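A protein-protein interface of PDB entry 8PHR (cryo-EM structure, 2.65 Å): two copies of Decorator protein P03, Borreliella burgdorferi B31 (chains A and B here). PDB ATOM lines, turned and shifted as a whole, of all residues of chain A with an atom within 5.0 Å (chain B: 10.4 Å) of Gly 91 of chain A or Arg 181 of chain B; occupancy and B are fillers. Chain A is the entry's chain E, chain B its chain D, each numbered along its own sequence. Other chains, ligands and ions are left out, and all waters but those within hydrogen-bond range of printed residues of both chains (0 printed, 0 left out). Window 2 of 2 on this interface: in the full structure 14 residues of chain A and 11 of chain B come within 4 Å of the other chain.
Among the printed residues, merely in contact across the chains: Gly 91 of chain A with Arg 181 of chain B, Asp 92 of chain A with Arg 181 of chain B and Tyr 95 of chain A with Ser 176 of chain B.
Among the printed residues, no Asp or Glu carboxylate lies within 4 Å of a Lys or Arg side-chain nitrogen of the other chain.
Of the printed residues of chain B, Gly 91 of chain A touches Arg 181 (3.9 Å).
Of chain A, only Gly 91, Asp 92, Leu 94 and Asn 180 come within 4 Å of Arg 181 of chain B.
Asp 92 of chain A touches one residue of chain B.
No residue of chain B comes within 4 Å of Asp 93 of chain A.
Leu 94 of chain A touches one residue of chain B.
Of the printed residues of chain A, Asn 180 of chain B touches Asn 180.
Printed residues of chain B within 4 Å of Tyr 95 of chain A: Ser 176 (3.7 Å).
Of the printed residues of chain B, Asn 180 of chain A touches Asn 180 (3.5 Å) and Arg 181 (3.3 Å).
Of the printed residues of chain A, Ser 176 of chain B touches Tyr 95 (3.7 Å).
The nearest residue of chain B that does not touch Gly 91 of chain A is Lys 136 of chain B (7.6 Å).
Asn 180 of chain B touches its own counterpart, Asn 180 of chain A.
The side-chain amide oxygen of Asn 180 of chain A is in hydrogen-bond range of the guanidinium group of Arg 181 of chain B, at 3.3 Å.
The backbone carbonyl oxygen of Asn 180 of chain B sits at hydrogen-bond distance from the side-chain amide nitrogen of Asn 180 of chain A, at 3.5 Å.
NH2 of Arg 181 of chain B lies within hydrogen-bond range of O of Leu 94 of chain A, 2.5 Å away.
The backbone NH (N) of Ser 176 of chain B sits at hydrogen-bond distance from the backbone carbonyl oxygen (O) of Ile 158 of chain B (3.1 Å).
The backbone NH (N) of Val 155 of chain B is in hydrogen-bond range of the backbone carbonyl oxygen (O) of Arg 181 of chain B (3.0 Å).
The side-chain amide oxygen (OD1) of Asn 156 of chain B lies close to the side-chain amide oxygen (OD1) of Asn 180 of chain B (3.2 Å).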
ATOM      1  N   GLY A  89      -5.906   9.703 -11.951  1.00  0.00           N
ATOM      2  CA  GLY A  89      -6.696  10.800 -11.424  1.00  0.00           C
ATOM      3  C   GLY A  89      -6.131  11.280 -10.107  1.00  0.00           C
ATOM      4  O   GLY A  89      -5.145  10.744  -9.593  1.00  0.00           O
ATOM      5  N   GLY A  90      -6.770  12.302  -9.570  1.00  0.00           N
ATOM      6  CA  GLY A  90      -6.365  12.876  -8.302  1.00  0.00           C
ATOM      7  C   GLY A  90      -7.468  13.707  -7.689  1.00  0.00           C
ATOM      8  O   GLY A  90      -8.652  13.379  -7.800  1.00  0.00           O
ATOM      9  N   GLY A  91      -7.074  14.794  -7.034  1.00  0.00           N
ATOM     10  CA  GLY A  91      -8.053  15.666  -6.403  1.00  0.00           C
ATOM     11  C   GLY A  91      -8.691  14.994  -5.203  1.00  0.00           C
ATOM     12  O   GLY A  91      -8.011  14.402  -4.358  1.00  0.00           O
ATOM     13  N   ASP A  92     -10.018  15.090  -5.118  1.00  0.00           N
ATOM     14  CA  ASP A  92     -10.754  14.505  -4.004  1.00  0.00           C
ATOM     15  C   ASP A  92     -11.030  13.020  -4.191  1.00  0.00           C
ATOM     16  O   ASP A  92     -11.536  12.380  -3.263  1.00  0.00           O
ATOM     17  CB  ASP A  92     -12.079  15.246  -3.804  1.00  0.00           C
ATOM     18  CG  ASP A  92     -11.886  16.663  -3.299  1.00  0.00           C
ATOM     19  OD1 ASP A  92     -10.723  17.078  -3.115  1.00  0.00           O
ATOM     20  OD2 ASP A  92     -12.899  17.362  -3.087  1.00  0.00           O
ATOM     21  N   ASP A  93     -10.715  12.460  -5.357  1.00  0.00           N
ATOM     22  CA  ASP A  93     -10.982  11.062  -5.656  1.00  0.00           C
ATOM     23  C   ASP A  93      -9.742  10.184  -5.537  1.00  0.00           C
ATOM     24  O   ASP A  93      -9.807   8.995  -5.862  1.00  0.00           O
ATOM     25  CB  ASP A  93     -11.578  10.929  -7.058  1.00  0.00           C
ATOM     26  CG  ASP A  93     -12.631  11.980  -7.345  1.00  0.00           C
ATOM     27  OD1 ASP A  93     -13.654  12.011  -6.629  1.00  0.00           O
ATOM     28  OD2 ASP A  93     -12.434  12.777  -8.285  1.00  0.00           O
ATOM     29  N   LEU A  94      -8.622  10.738  -5.076  1.00  0.00           N
ATOM     30  CA  LEU A  94      -7.374   9.987  -5.034  1.00  0.00           C
ATOM     31  C   LEU A  94      -7.485   8.810  -4.074  1.00  0.00           C
ATOM     32  O   LEU A  94      -7.752   8.989  -2.881  1.00  0.00           O
ATOM     33  CB  LEU A  94      -6.223  10.902  -4.619  1.00  0.00           C
ATOM     34  CG  LEU A  94      -4.838  10.251  -4.603  1.00  0.00           C
ATOM     35  CD1 LEU A  94      -4.331  10.025  -6.021  1.00  0.00           C
ATOM     36  CD2 LEU A  94      -3.852  11.085  -3.802  1.00  0.00           C
ATOM     37  N   TYR A  95      -7.282   7.604  -4.600  1.00  0.00           N
ATOM     38  CA  TYR A  95      -7.320   6.387  -3.801  1.00  0.00           C
ATOM     39  C   TYR A  95      -5.936   5.869  -3.435  1.00  0.00           C
ATOM     40  O   TYR A  95      -5.775   5.272  -2.366  1.00  0.00           O
ATOM     41  CB  TYR A  95      -8.087   5.289  -4.547  1.00  0.00           C
ATOM     42  CG  TYR A  95      -8.142   3.967  -3.817  1.00  0.00           C
ATOM     43  CD1 TYR A  95      -8.921   3.813  -2.677  1.00  0.00           C
ATOM     44  CD2 TYR A  95      -7.416   2.871  -4.266  1.00  0.00           C
ATOM     45  CE1 TYR A  95      -8.974   2.606  -2.006  1.00  0.00           C
ATOM     46  CE2 TYR A  95      -7.463   1.661  -3.602  1.00  0.00           C
ATOM     47  CZ  TYR A  95      -8.244   1.534  -2.473  1.00  0.00           C
ATOM     48  OH  TYR A  95      -8.293   0.330  -1.807  1.00  0.00           O
ATOM     49  N   PHE A 139      -1.532  16.069  -6.487  1.00  0.00           N
ATOM     50  CA  PHE A 139      -1.928  15.353  -7.692  1.00  0.00           C
ATOM     51  C   PHE A 139      -3.016  16.117  -8.435  1.00  0.00           C
ATOM     52  O   PHE A 139      -3.900  16.724  -7.821  1.00  0.00           O
ATOM     53  CB  PHE A 139      -2.419  13.949  -7.339  1.00  0.00           C
ATOM     54  CG  PHE A 139      -1.311  12.975  -7.055  1.00  0.00           C
ATOM     55  CD1 PHE A 139      -0.465  12.552  -8.067  1.00  0.00           C
ATOM     56  CD2 PHE A 139      -1.113  12.485  -5.775  1.00  0.00           C
ATOM     57  CE1 PHE A 139       0.555  11.657  -7.809  1.00  0.00           C
ATOM     58  CE2 PHE A 139      -0.094  11.590  -5.509  1.00  0.00           C
ATOM     59  CZ  PHE A 139       0.740  11.176  -6.527  1.00  0.00           C
ATOM     60  N   ASN A 140      -2.950  16.085  -9.762  1.00  0.00           N
ATOM     61  CA  ASN A 140      -3.921  16.763 -10.605  1.00  0.00           C
ATOM     62  C   ASN A 140      -4.952  15.763 -11.129  1.00  0.00           C
ATOM     63  O   ASN A 140      -4.994  14.601 -10.713  1.00  0.00           O
ATOM     64  CB  ASN A 140      -3.206  17.506 -11.739  1.00  0.00           C
ATOM     65  CG  ASN A 140      -2.488  16.571 -12.701  1.00  0.00           C
ATOM     66  OD1 ASN A 140      -2.475  15.354 -12.519  1.00  0.00           O
ATOM     67  ND2 ASN A 140      -1.887  17.145 -13.737  1.00  0.00           N
ATOM     68  N   SER A 154      -4.676  19.063  -0.271  1.00  0.00           N
ATOM     69  CA  SER A 154      -5.374  17.959   0.374  1.00  0.00           C
ATOM     70  C   SER A 154      -4.535  16.699   0.516  1.00  0.00           C
ATOM     71  O   SER A 154      -4.940  15.796   1.257  1.00  0.00           O
ATOM     72  CB  SER A 154      -6.658  17.612  -0.396  1.00  0.00           C
ATOM     73  OG  SER A 154      -6.360  17.154  -1.703  1.00  0.00           O
ATOM     74  N   VAL A 155      -3.392  16.605  -0.158  1.00  0.00           N
ATOM     75  CA  VAL A 155      -2.526  15.434  -0.097  1.00  0.00           C
ATOM     76  C   VAL A 155      -1.122  15.898   0.261  1.00  0.00           C
ATOM     77  O   VAL A 155      -0.601  16.838  -0.350  1.00  0.00           O
ATOM     78  CB  VAL A 155      -2.520  14.657  -1.429  1.00  0.00           C
ATOM     79  CG1 VAL A 155      -1.501  13.528  -1.384  1.00  0.00           C
ATOM     80  CG2 VAL A 155      -3.908  14.118  -1.734  1.00  0.00           C
ATOM     81  N   ASN A 180      -3.209  12.062   3.546  1.00  0.00           N
ATOM     82  CA  ASN A 180      -3.965  13.286   3.330  1.00  0.00           C
ATOM     83  C   ASN A 180      -3.715  14.281   4.457  1.00  0.00           C
ATOM     84  O   ASN A 180      -3.363  13.908   5.579  1.00  0.00           O
ATOM     85  CB  ASN A 180      -5.461  12.985   3.231  1.00  0.00           C
ATOM     86  CG  ASN A 180      -5.769  11.868   2.256  1.00  0.00           C
ATOM     87  OD1 ASN A 180      -5.515  11.987   1.058  1.00  0.00           O
ATOM     88  ND2 ASN A 180      -6.322  10.773   2.765  1.00  0.00           N
ATOM     89  N   GLY B  91     -18.256  10.717  13.104  1.00  0.00           N
ATOM     90  CA  GLY B  91     -17.990  12.144  13.115  1.00  0.00           C
ATOM     91  C   GLY B  91     -16.515  12.446  13.321  1.00  0.00           C
ATOM     92  O   GLY B  91     -15.633  11.682  12.925  1.00  0.00           O
ATOM     93  N   ASP B  92     -16.250  13.592  13.953  1.00  0.00           N
ATOM     94  CA  ASP B  92     -14.875  13.987  14.235  1.00  0.00           C
ATOM     95  C   ASP B  92     -14.234  13.124  15.314  1.00  0.00           C
ATOM     96  O   ASP B  92     -13.007  13.148  15.460  1.00  0.00           O
ATOM     97  CB  ASP B  92     -14.822  15.458  14.650  1.00  0.00           C
ATOM     98  CG  ASP B  92     -15.502  16.371  13.649  1.00  0.00           C
ATOM     99  OD1 ASP B  92     -15.055  16.417  12.484  1.00  0.00           O
ATOM    100  OD2 ASP B  92     -16.483  17.045  14.028  1.00  0.00           O
ATOM    101  N   LEU B  94     -14.403   9.810  15.356  1.00  0.00           N
ATOM    102  CA  LEU B  94     -14.187   8.465  14.841  1.00  0.00           C
ATOM    103  C   LEU B  94     -12.735   8.042  15.024  1.00  0.00           C
ATOM    104  O   LEU B  94     -11.809   8.796  14.712  1.00  0.00           O
ATOM    105  CB  LEU B  94     -14.575   8.399  13.363  1.00  0.00           C
ATOM    106  CG  LEU B  94     -14.215   7.114  12.616  1.00  0.00           C
ATOM    107  CD1 LEU B  94     -15.295   6.061  12.804  1.00  0.00           C
ATOM    108  CD2 LEU B  94     -13.987   7.396  11.140  1.00  0.00           C
ATOM    109  N   ILE B 113      -8.382   3.930  11.823  1.00  0.00           N
ATOM    110  CA  ILE B 113      -8.678   4.760  10.659  1.00  0.00           C
ATOM    111  C   ILE B 113      -7.430   4.960   9.807  1.00  0.00           C
ATOM    112  O   ILE B 113      -7.525   5.215   8.600  1.00  0.00           O
ATOM    113  CB  ILE B 113      -9.289   6.103  11.106  1.00  0.00           C
ATOM    114  CG1 ILE B 113      -9.852   6.870   9.907  1.00  0.00           C
ATOM    115  CG2 ILE B 113      -8.261   6.945  11.851  1.00  0.00           C
ATOM    116  CD1 ILE B 113     -10.999   6.165   9.221  1.00  0.00           C
ATOM    117  N   LYS B 136     -20.399   8.652  -1.879  1.00  0.00           N
ATOM    118  CA  LYS B 136     -19.515   8.984  -0.771  1.00  0.00           C
ATOM    119  C   LYS B 136     -20.274   8.838   0.541  1.00  0.00           C
ATOM    120  O   LYS B 136     -21.370   9.387   0.694  1.00  0.00           O
ATOM    121  CB  LYS B 136     -18.971  10.405  -0.920  1.00  0.00           C
ATOM    122  CG  LYS B 136     -18.136  10.610  -2.174  1.00  0.00           C
ATOM    123  CD  LYS B 136     -17.514  11.997  -2.212  1.00  0.00           C
ATOM    124  CE  LYS B 136     -16.590  12.153  -3.409  1.00  0.00           C
ATOM    125  NZ  LYS B 136     -15.921  13.484  -3.435  1.00  0.00           N
ATOM    126  N   LEU B 137     -19.688   8.100   1.482  1.00  0.00           N
ATOM    127  CA  LEU B 137     -20.338   7.752   2.736  1.00  0.00           C
ATOM    128  C   LEU B 137     -19.496   8.221   3.914  1.00  0.00           C
ATOM    129  O   LEU B 137     -18.264   8.120   3.890  1.00  0.00           O
ATOM    130  CB  LEU B 137     -20.565   6.240   2.833  1.00  0.00           C
ATOM    131  CG  LEU B 137     -21.365   5.582   1.708  1.00  0.00           C
ATOM    132  CD1 LEU B 137     -21.660   4.127   2.042  1.00  0.00           C
ATOM    133  CD2 LEU B 137     -22.651   6.344   1.440  1.00  0.00           C
ATOM    134  N   ASN B 138     -20.172   8.731   4.940  1.00  0.00           N
ATOM    135  CA  ASN B 138     -19.542   9.155   6.181  1.00  0.00           C
ATOM    136  C   ASN B 138     -20.283   8.534   7.357  1.00  0.00           C
ATOM    137  O   ASN B 138     -21.473   8.218   7.265  1.00  0.00           O
ATOM    138  CB  ASN B 138     -19.528  10.685   6.318  1.00  0.00           C
ATOM    139  CG  ASN B 138     -20.921  11.271   6.435  1.00  0.00           C
ATOM    140  OD1 ASN B 138     -21.734  11.156   5.518  1.00  0.00           O
ATOM    141  ND2 ASN B 138     -21.203  11.911   7.565  1.00  0.00           N
ATOM    142  N   PHE B 139     -19.566   8.357   8.464  1.00  0.00           N
ATOM    143  CA  PHE B 139     -20.148   7.753   9.654  1.00  0.00           C
ATOM    144  C   PHE B 139     -20.947   8.783  10.441  1.00  0.00           C
ATOM    145  O   PHE B 139     -20.530   9.935  10.589  1.00  0.00           O
ATOM    146  CB  PHE B 139     -19.051   7.152  10.533  1.00  0.00           C
ATOM    147  CG  PHE B 139     -18.549   5.822  10.048  1.00  0.00           C
ATOM    148  CD1 PHE B 139     -19.334   4.686  10.159  1.00  0.00           C
ATOM    149  CD2 PHE B 139     -17.293   5.709   9.474  1.00  0.00           C
ATOM    150  CE1 PHE B 139     -18.874   3.463   9.711  1.00  0.00           C
ATOM    151  CE2 PHE B 139     -16.828   4.487   9.024  1.00  0.00           C
ATOM    152  CZ  PHE B 139     -17.619   3.363   9.143  1.00  0.00           C
ATOM    153  N   VAL B 148     -23.088  11.429   2.037  1.00  0.00           N
ATOM    154  CA  VAL B 148     -22.624  12.771   2.364  1.00  0.00           C
ATOM    155  C   VAL B 148     -23.510  13.817   1.699  1.00  0.00           C
ATOM    156  O   VAL B 148     -23.968  13.630   0.572  1.00  0.00           O
ATOM    157  CB  VAL B 148     -21.154  12.965   1.955  1.00  0.00           C
ATOM    158  CG1 VAL B 148     -20.693  14.376   2.285  1.00  0.00           C
ATOM    159  CG2 VAL B 148     -20.270  11.933   2.641  1.00  0.00           C
ATOM    160  N   SER B 154     -16.565  16.079   5.145  1.00  0.00           N
ATOM    161  CA  SER B 154     -15.638  14.969   5.322  1.00  0.00           C
ATOM    162  C   SER B 154     -16.216  13.694   4.725  1.00  0.00           C
ATOM    163  O   SER B 154     -17.384  13.370   4.937  1.00  0.00           O
ATOM    164  CB  SER B 154     -15.317  14.764   6.805  1.00  0.00           C
ATOM    165  OG  SER B 154     -14.466  13.646   6.997  1.00  0.00           O
ATOM    166  N   VAL B 155     -15.388  12.972   3.975  1.00  0.00           N
ATOM    167  CA  VAL B 155     -15.777  11.727   3.328  1.00  0.00           C
ATOM    168  C   VAL B 155     -14.908  10.611   3.891  1.00  0.00           C
ATOM    169  O   VAL B 155     -13.679  10.748   3.955  1.00  0.00           O
ATOM    170  CB  VAL B 155     -15.637  11.814   1.797  1.00  0.00           C
ATOM    171  CG1 VAL B 155     -16.007  10.492   1.152  1.00  0.00           C
ATOM    172  CG2 VAL B 155     -16.495  12.945   1.240  1.00  0.00           C
ATOM    173  N   ASN B 156     -15.544   9.504   4.286  1.00  0.00           N
ATOM    174  CA  ASN B 156     -14.844   8.402   4.930  1.00  0.00           C
ATOM    175  C   ASN B 156     -14.767   7.132   4.096  1.00  0.00           C
ATOM    176  O   ASN B 156     -13.827   6.354   4.289  1.00  0.00           O
ATOM    177  CB  ASN B 156     -15.502   8.061   6.278  1.00  0.00           C
ATOM    178  CG  ASN B 156     -15.285   9.139   7.330  1.00  0.00           C
ATOM    179  OD1 ASN B 156     -14.192   9.696   7.461  1.00  0.00           O
ATOM    180  ND2 ASN B 156     -16.338   9.445   8.081  1.00  0.00           N
ATOM    181  N   ALA B 157     -15.709   6.892   3.185  1.00  0.00           N
ATOM    182  CA  ALA B 157     -15.687   5.667   2.396  1.00  0.00           C
ATOM    183  C   ALA B 157     -16.413   5.890   1.078  1.00  0.00           C
ATOM    184  O   ALA B 157     -17.133   6.875   0.894  1.00  0.00           O
ATOM    185  CB  ALA B 157     -16.310   4.497   3.166  1.00  0.00           C
ATOM    186  N   ILE B 158     -16.226   4.946   0.159  1.00  0.00           N
ATOM    187  CA  ILE B 158     -16.902   4.947  -1.133  1.00  0.00           C
ATOM    188  C   ILE B 158     -17.688   3.649  -1.248  1.00  0.00           C
ATOM    189  O   ILE B 158     -17.128   2.562  -1.067  1.00  0.00           O
ATOM    190  CB  ILE B 158     -15.903   5.096  -2.297  1.00  0.00           C
ATOM    191  CG1 ILE B 158     -15.368   6.529  -2.349  1.00  0.00           C
ATOM    192  CG2 ILE B 158     -16.552   4.712  -3.620  1.00  0.00           C
ATOM    193  CD1 ILE B 158     -14.429   6.796  -3.505  1.00  0.00           C
ATOM    194  N   SER B 176     -15.389   0.913   0.884  1.00  0.00           N
ATOM    195  CA  SER B 176     -13.934   0.970   0.971  1.00  0.00           C
ATOM    196  C   SER B 176     -13.555   2.217   1.759  1.00  0.00           C
ATOM    197  O   SER B 176     -13.753   3.340   1.284  1.00  0.00           O
ATOM    198  CB  SER B 176     -13.299   0.981  -0.419  1.00  0.00           C
ATOM    199  OG  SER B 176     -11.885   1.019  -0.334  1.00  0.00           O
ATOM    200  N   VAL B 177     -13.002   2.021   2.952  1.00  0.00           N
ATOM    201  CA  VAL B 177     -12.634   3.122   3.834  1.00  0.00           C
ATOM    202  C   VAL B 177     -11.196   3.527   3.543  1.00  0.00           C
ATOM    203  O   VAL B 177     -10.301   2.675   3.485  1.00  0.00           O
ATOM    204  CB  VAL B 177     -12.808   2.727   5.309  1.00  0.00           C
ATOM    205  CG1 VAL B 177     -12.665   3.945   6.205  1.00  0.00           C
ATOM    206  CG2 VAL B 177     -14.158   2.056   5.522  1.00  0.00           C
ATOM    207  N   PHE B 178     -10.973   4.825   3.355  1.00  0.00           N
ATOM    208  CA  PHE B 178      -9.653   5.365   3.049  1.00  0.00           C
ATOM    209  C   PHE B 178      -9.309   6.527   3.972  1.00  0.00           C
ATOM    210  O   PHE B 178      -8.653   7.493   3.569  1.00  0.00           O
ATOM    211  CB  PHE B 178      -9.555   5.774   1.579  1.00  0.00           C
ATOM    212  CG  PHE B 178     -10.620   6.741   1.138  1.00  0.00           C
ATOM    213  CD1 PHE B 178     -11.826   6.276   0.642  1.00  0.00           C
ATOM    214  CD2 PHE B 178     -10.410   8.110   1.196  1.00  0.00           C
ATOM    215  CE1 PHE B 178     -12.810   7.154   0.228  1.00  0.00           C
ATOM    216  CE2 PHE B 178     -11.390   8.994   0.782  1.00  0.00           C
ATOM    217  CZ  PHE B 178     -12.590   8.515   0.296  1.00  0.00           C
ATOM    218  N   GLY B 179      -9.729   6.445   5.232  1.00  0.00           N
ATOM    219  CA  GLY B 179      -9.311   7.431   6.211  1.00  0.00           C
ATOM    220  C   GLY B 179     -10.108   8.725   6.140  1.00  0.00           C
ATOM    221  O   GLY B 179     -11.289   8.746   5.784  1.00  0.00           O
ATOM    222  N   ASN B 180      -9.436   9.821   6.488  1.00  0.00           N
ATOM    223  CA  ASN B 180     -10.060  11.130   6.609  1.00  0.00           C
ATOM    224  C   ASN B 180      -9.586  12.049   5.490  1.00  0.00           C
ATOM    225  O   ASN B 180      -8.388  12.119   5.195  1.00  0.00           O
ATOM    226  CB  ASN B 180      -9.733  11.768   7.963  1.00  0.00           C
ATOM    227  CG  ASN B 180     -10.418  11.069   9.122  1.00  0.00           C
ATOM    228  OD1 ASN B 180     -11.589  10.697   9.032  1.00  0.00           O
ATOM    229  ND2 ASN B 180      -9.695  10.891  10.220  1.00  0.00           N
ATOM    230  N   ARG B 181     -10.536  12.749   4.871  1.00  0.00           N
ATOM    231  CA  ARG B 181     -10.233  13.739   3.846  1.00  0.00           C
ATOM    232  C   ARG B 181     -11.477  14.583   3.605  1.00  0.00           C
ATOM    233  O   ARG B 181     -12.592  14.056   3.569  1.00  0.00           O
ATOM    234  CB  ARG B 181      -9.768  13.083   2.539  1.00  0.00           C
ATOM    235  CG  ARG B 181      -9.369  14.077   1.454  1.00  0.00           C
ATOM    236  CD  ARG B 181      -8.587  13.414   0.324  1.00  0.00           C
ATOM    237  NE  ARG B 181      -9.216  12.191  -0.161  1.00  0.00           N
ATOM    238  CZ  ARG B 181      -8.671  11.374  -1.053  1.00  0.00           C
ATOM    239  NH1 ARG B 181      -7.492  11.629  -1.594  1.00  0.00           N
ATOM    240  NH2 ARG B 181      -9.327  10.274  -1.413  1.00  0.00           N
ATOM    241  N   ALA B 182     -11.278  15.889   3.450  1.00  0.00           N
ATOM    242  CA  ALA B 182     -12.382  16.801   3.167  1.00  0.00           C
ATOM    243  C   ALA B 182     -12.672  16.841   1.671  1.00  0.00           C
ATOM    244  O   ALA B 182     -13.819  16.998   1.254  1.00  0.00           O
ATOM    245  CB  ALA B 182     -12.070  18.195   3.688  1.00  0.00           C
